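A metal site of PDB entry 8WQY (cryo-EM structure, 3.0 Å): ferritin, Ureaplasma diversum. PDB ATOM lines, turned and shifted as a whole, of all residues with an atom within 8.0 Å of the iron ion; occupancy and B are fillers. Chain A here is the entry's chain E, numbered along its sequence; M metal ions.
OD2 of Asp 138 lies close to NE2 of His 65, 2.9 Å away. NZ of Lys 61 sits close to OD2 of Asp 142.
The iron ion is bound by OD2 of Asp 138, OD2 of Asp 142 and OD2 of Asp 60. The iron ion has three donor atoms within binding distance. Slightly farther from the iron ion lies the side-chain carboxylate (OD1) of Asp 142 (2.8 Å). Slightly farther from the iron ion lies a ring nitrogen (NE2) of His 65 (2.8 Å).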
ATOM      1  N   HIS A  56      18.404   4.283   5.502  1.00  0.00           N
ATOM      2  CA  HIS A  56      19.683   3.852   4.932  1.00  0.00           C
ATOM      3  C   HIS A  56      19.876   4.440   3.549  1.00  0.00           C
ATOM      4  O   HIS A  56      20.974   4.893   3.198  1.00  0.00           O
ATOM      5  CB  HIS A  56      19.755   2.328   4.888  1.00  0.00           C
ATOM      6  CG  HIS A  56      21.109   1.801   4.499  1.00  0.00           C
ATOM      7  ND1 HIS A  56      21.927   1.132   5.381  1.00  0.00           N
ATOM      8  CD2 HIS A  56      21.768   1.839   3.328  1.00  0.00           C
ATOM      9  CE1 HIS A  56      23.044   0.784   4.777  1.00  0.00           C
ATOM     10  NE2 HIS A  56      22.969   1.198   3.521  1.00  0.00           N
ATOM     11  N   LEU A  57      18.810   4.455   2.745  1.00  0.00           N
ATOM     12  CA  LEU A  57      18.938   4.994   1.394  1.00  0.00           C
ATOM     13  C   LEU A  57      19.221   6.491   1.432  1.00  0.00           C
ATOM     14  O   LEU A  57      20.023   7.012   0.643  1.00  0.00           O
ATOM     15  CB  LEU A  57      17.687   4.692   0.592  1.00  0.00           C
ATOM     16  CG  LEU A  57      17.829   4.664  -0.934  1.00  0.00           C
ATOM     17  CD1 LEU A  57      16.756   3.774  -1.522  1.00  0.00           C
ATOM     18  CD2 LEU A  57      17.754   6.045  -1.531  1.00  0.00           C
ATOM     19  N   ASP A  60      22.819   7.068   2.374  1.00  0.00           N
ATOM     20  CA  ASP A  60      23.657   6.782   1.221  1.00  0.00           C
ATOM     21  C   ASP A  60      23.630   7.910   0.206  1.00  0.00           C
ATOM     22  O   ASP A  60      24.636   8.184  -0.442  1.00  0.00           O
ATOM     23  CB  ASP A  60      23.214   5.468   0.584  1.00  0.00           C
ATOM     24  CG  ASP A  60      23.914   5.195  -0.727  1.00  0.00           C
ATOM     25  OD1 ASP A  60      25.127   5.496  -0.831  1.00  0.00           O
ATOM     26  OD2 ASP A  60      23.268   4.668  -1.653  1.00  0.00           O
ATOM     27  N   LYS A  61      22.478   8.577   0.050  1.00  0.00           N
ATOM     28  CA  LYS A  61      22.421   9.705  -0.875  1.00  0.00           C
ATOM     29  C   LYS A  61      23.147  10.923  -0.317  1.00  0.00           C
ATOM     30  O   LYS A  61      23.742  11.690  -1.081  1.00  0.00           O
ATOM     31  CB  LYS A  61      20.971  10.066  -1.188  1.00  0.00           C
ATOM     32  CG  LYS A  61      20.251   9.057  -2.050  1.00  0.00           C
ATOM     33  CD  LYS A  61      20.795   9.041  -3.459  1.00  0.00           C
ATOM     34  CE  LYS A  61      20.311   7.802  -4.193  1.00  0.00           C
ATOM     35  NZ  LYS A  61      20.810   7.722  -5.586  1.00  0.00           N
ATOM     36  N   VAL A  64      28.342   9.452   0.208  1.00  0.00           N
ATOM     37  CA  VAL A  64      29.311   9.319  -0.871  1.00  0.00           C
ATOM     38  C   VAL A  64      28.836   9.983  -2.152  1.00  0.00           C
ATOM     39  O   VAL A  64      29.639  10.535  -2.907  1.00  0.00           O
ATOM     40  CB  VAL A  64      29.639   7.821  -1.093  1.00  0.00           C
ATOM     41  CG1 VAL A  64      30.016   7.182   0.222  1.00  0.00           C
ATOM     42  CG2 VAL A  64      28.460   7.088  -1.696  1.00  0.00           C
ATOM     43  N   HIS A  65      27.513   9.977  -2.394  1.00  0.00           N
ATOM     44  CA  HIS A  65      26.977  10.499  -3.647  1.00  0.00           C
ATOM     45  C   HIS A  65      27.218  11.994  -3.812  1.00  0.00           C
ATOM     46  O   HIS A  65      26.993  12.516  -4.908  1.00  0.00           O
ATOM     47  CB  HIS A  65      25.489  10.210  -3.734  1.00  0.00           C
ATOM     48  CG  HIS A  65      25.156   8.808  -4.156  1.00  0.00           C
ATOM     49  ND1 HIS A  65      24.397   8.524  -5.264  1.00  0.00           N
ATOM     50  CD2 HIS A  65      25.492   7.623  -3.611  1.00  0.00           C
ATOM     51  CE1 HIS A  65      24.269   7.213  -5.384  1.00  0.00           C
ATOM     52  NE2 HIS A  65      24.926   6.638  -4.389  1.00  0.00           N
ATOM     53  N   GLU A 106      14.118   7.543  -8.199  1.00  0.00           N
ATOM     54  CA  GLU A 106      15.312   6.852  -8.681  1.00  0.00           C
ATOM     55  C   GLU A 106      15.318   6.743 -10.202  1.00  0.00           C
ATOM     56  O   GLU A 106      16.360   6.880 -10.859  1.00  0.00           O
ATOM     57  CB  GLU A 106      15.430   5.478  -8.033  1.00  0.00           C
ATOM     58  CG  GLU A 106      15.448   5.499  -6.525  1.00  0.00           C
ATOM     59  CD  GLU A 106      16.609   6.303  -5.971  1.00  0.00           C
ATOM     60  OE1 GLU A 106      17.684   6.301  -6.591  1.00  0.00           O
ATOM     61  OE2 GLU A 106      16.439   6.921  -4.906  1.00  0.00           O
ATOM     62  N   TRP A 134      30.359   5.438 -12.476  1.00  0.00           N
ATOM     63  CA  TRP A 134      30.292   4.876 -11.167  1.00  0.00           C
ATOM     64  C   TRP A 134      28.885   5.128 -10.903  1.00  0.00           C
ATOM     65  O   TRP A 134      28.191   4.331 -10.326  1.00  0.00           O
ATOM     66  CB  TRP A 134      31.122   5.665 -10.177  1.00  0.00           C
ATOM     67  CG  TRP A 134      31.127   5.124  -8.784  1.00  0.00           C
ATOM     68  CD1 TRP A 134      31.985   4.195  -8.279  1.00  0.00           C
ATOM     69  CD2 TRP A 134      30.265   5.499  -7.703  1.00  0.00           C
ATOM     70  NE1 TRP A 134      31.699   3.957  -6.952  1.00  0.00           N
ATOM     71  CE2 TRP A 134      30.642   4.749  -6.587  1.00  0.00           C
ATOM     72  CE3 TRP A 134      29.203   6.400  -7.582  1.00  0.00           C
ATOM     73  CZ2 TRP A 134      29.986   4.843  -5.375  1.00  0.00           C
ATOM     74  CZ3 TRP A 134      28.565   6.493  -6.384  1.00  0.00           C
ATOM     75  CH2 TRP A 134      28.954   5.734  -5.288  1.00  0.00           C
ATOM     76  N   TYR A 135      28.428   6.261 -11.378  1.00  0.00           N
ATOM     77  CA  TYR A 135      27.022   6.595 -11.197  1.00  0.00           C
ATOM     78  C   TYR A 135      26.136   5.777 -12.132  1.00  0.00           C
ATOM     79  O   TYR A 135      25.021   5.411 -11.754  1.00  0.00           O
ATOM     80  CB  TYR A 135      26.812   8.083 -11.398  1.00  0.00           C
ATOM     81  CG  TYR A 135      27.443   8.915 -10.307  1.00  0.00           C
ATOM     82  CD1 TYR A 135      26.747   9.225  -9.160  1.00  0.00           C
ATOM     83  CD2 TYR A 135      28.743   9.378 -10.431  1.00  0.00           C
ATOM     84  CE1 TYR A 135      27.314   9.974  -8.167  1.00  0.00           C
ATOM     85  CE2 TYR A 135      29.314  10.128  -9.446  1.00  0.00           C
ATOM     86  CZ  TYR A 135      28.602  10.430  -8.312  1.00  0.00           C
ATOM     87  OH  TYR A 135      29.169  11.178  -7.319  1.00  0.00           O
ATOM     88  N   ARG A 137      26.501   2.757 -12.860  1.00  0.00           N
ATOM     89  CA  ARG A 137      26.304   1.466 -12.227  1.00  0.00           C
ATOM     90  C   ARG A 137      25.477   1.573 -10.955  1.00  0.00           C
ATOM     91  O   ARG A 137      24.567   0.769 -10.719  1.00  0.00           O
ATOM     92  CB  ARG A 137      27.660   0.829 -11.919  1.00  0.00           C
ATOM     93  CG  ARG A 137      27.610  -0.304 -10.927  1.00  0.00           C
ATOM     94  CD  ARG A 137      28.998  -0.626 -10.411  1.00  0.00           C
ATOM     95  NE  ARG A 137      29.530   0.451  -9.578  1.00  0.00           N
ATOM     96  CZ  ARG A 137      29.188   0.638  -8.311  1.00  0.00           C
ATOM     97  NH1 ARG A 137      28.320  -0.174  -7.732  1.00  0.00           N
ATOM     98  NH2 ARG A 137      29.716   1.638  -7.624  1.00  0.00           N
ATOM     99  N   ASP A 138      25.783   2.573 -10.121  1.00  0.00           N
ATOM    100  CA  ASP A 138      25.072   2.715  -8.867  1.00  0.00           C
ATOM    101  C   ASP A 138      23.607   3.063  -9.085  1.00  0.00           C
ATOM    102  O   ASP A 138      22.767   2.704  -8.258  1.00  0.00           O
ATOM    103  CB  ASP A 138      25.747   3.771  -7.993  1.00  0.00           C
ATOM    104  CG  ASP A 138      25.478   3.577  -6.524  1.00  0.00           C
ATOM    105  OD1 ASP A 138      26.144   2.719  -5.906  1.00  0.00           O
ATOM    106  OD2 ASP A 138      24.601   4.272  -5.976  1.00  0.00           O
ATOM    107  N   GLY A 139      23.274   3.726 -10.189  1.00  0.00           N
ATOM    108  CA  GLY A 139      21.877   4.019 -10.468  1.00  0.00           C
ATOM    109  C   GLY A 139      21.058   2.757 -10.687  1.00  0.00           C
ATOM    110  O   GLY A 139      19.980   2.597 -10.105  1.00  0.00           O
ATOM    111  N   LEU A 140      21.574   1.845 -11.508  1.00  0.00           N
ATOM    112  CA  LEU A 140      20.866   0.586 -11.734  1.00  0.00           C
ATOM    113  C   LEU A 140      20.842  -0.266 -10.475  1.00  0.00           C
ATOM    114  O   LEU A 140      19.840  -0.932 -10.179  1.00  0.00           O
ATOM    115  CB  LEU A 140      21.503  -0.183 -12.884  1.00  0.00           C
ATOM    116  CG  LEU A 140      20.590  -1.221 -13.520  1.00  0.00           C
ATOM    117  CD1 LEU A 140      19.393  -0.533 -14.138  1.00  0.00           C
ATOM    118  CD2 LEU A 140      21.324  -2.026 -14.565  1.00  0.00           C
ATOM    119  N   LYS A 141      21.940  -0.276  -9.711  1.00  0.00           N
ATOM    120  CA  LYS A 141      21.948  -1.031  -8.465  1.00  0.00           C
ATOM    121  C   LYS A 141      20.876  -0.523  -7.513  1.00  0.00           C
ATOM    122  O   LYS A 141      20.094  -1.306  -6.958  1.00  0.00           O
ATOM    123  CB  LYS A 141      23.328  -0.955  -7.811  1.00  0.00           C
ATOM    124  CG  LYS A 141      23.326  -1.367  -6.360  1.00  0.00           C
ATOM    125  CD  LYS A 141      24.496  -0.765  -5.611  1.00  0.00           C
ATOM    126  CE  LYS A 141      24.204  -0.688  -4.121  1.00  0.00           C
ATOM    127  NZ  LYS A 141      25.404  -0.267  -3.349  1.00  0.00           N
ATOM    128  N   ASP A 142      20.804   0.805  -7.313  1.00  0.00           N
ATOM    129  CA  ASP A 142      19.826   1.362  -6.399  1.00  0.00           C
ATOM    130  C   ASP A 142      18.403   1.147  -6.905  1.00  0.00           C
ATOM    131  O   ASP A 142      17.493   0.903  -6.108  1.00  0.00           O
ATOM    132  CB  ASP A 142      20.098   2.848  -6.191  1.00  0.00           C
ATOM    133  CG  ASP A 142      21.213   3.100  -5.184  1.00  0.00           C
ATOM    134  OD1 ASP A 142      21.644   2.140  -4.518  1.00  0.00           O
ATOM    135  OD2 ASP A 142      21.658   4.258  -5.070  1.00  0.00           O
ATOM    136  N   LEU A 143      18.195   1.234  -8.216  1.00  0.00           N
ATOM    137  CA  LEU A 143      16.863   0.971  -8.755  1.00  0.00           C
ATOM    138  C   LEU A 143      16.433  -0.471  -8.493  1.00  0.00           C
ATOM    139  O   LEU A 143      15.294  -0.719  -8.068  1.00  0.00           O
ATOM    140  CB  LEU A 143      16.838   1.254 -10.249  1.00  0.00           C
ATOM    141  CG  LEU A 143      15.444   1.115 -10.857  1.00  0.00           C
ATOM    142  CD1 LEU A 143      14.591   2.300 -10.484  1.00  0.00           C
ATOM    143  CD2 LEU A 143      15.515   0.934 -12.350  1.00  0.00           C
ATOM    144  N   GLU A 145      17.455  -2.382  -6.157  1.00  0.00           N
ATOM    145  CA  GLU A 145      17.221  -2.582  -4.730  1.00  0.00           C
ATOM    146  C   GLU A 145      15.880  -1.993  -4.303  1.00  0.00           C
ATOM    147  O   GLU A 145      15.164  -2.595  -3.490  1.00  0.00           O
ATOM    148  CB  GLU A 145      18.356  -1.963  -3.912  1.00  0.00           C
ATOM    149  CG  GLU A 145      19.404  -2.965  -3.474  1.00  0.00           C
ATOM    150  CD  GLU A 145      20.521  -2.330  -2.685  1.00  0.00           C
ATOM    151  OE1 GLU A 145      20.432  -1.116  -2.398  1.00  0.00           O
ATOM    152  OE2 GLU A 145      21.493  -3.044  -2.349  1.00  0.00           O
HETATM  153 FE    FE M   1      23.670   4.098  -4.157  1.00  0.00          FE
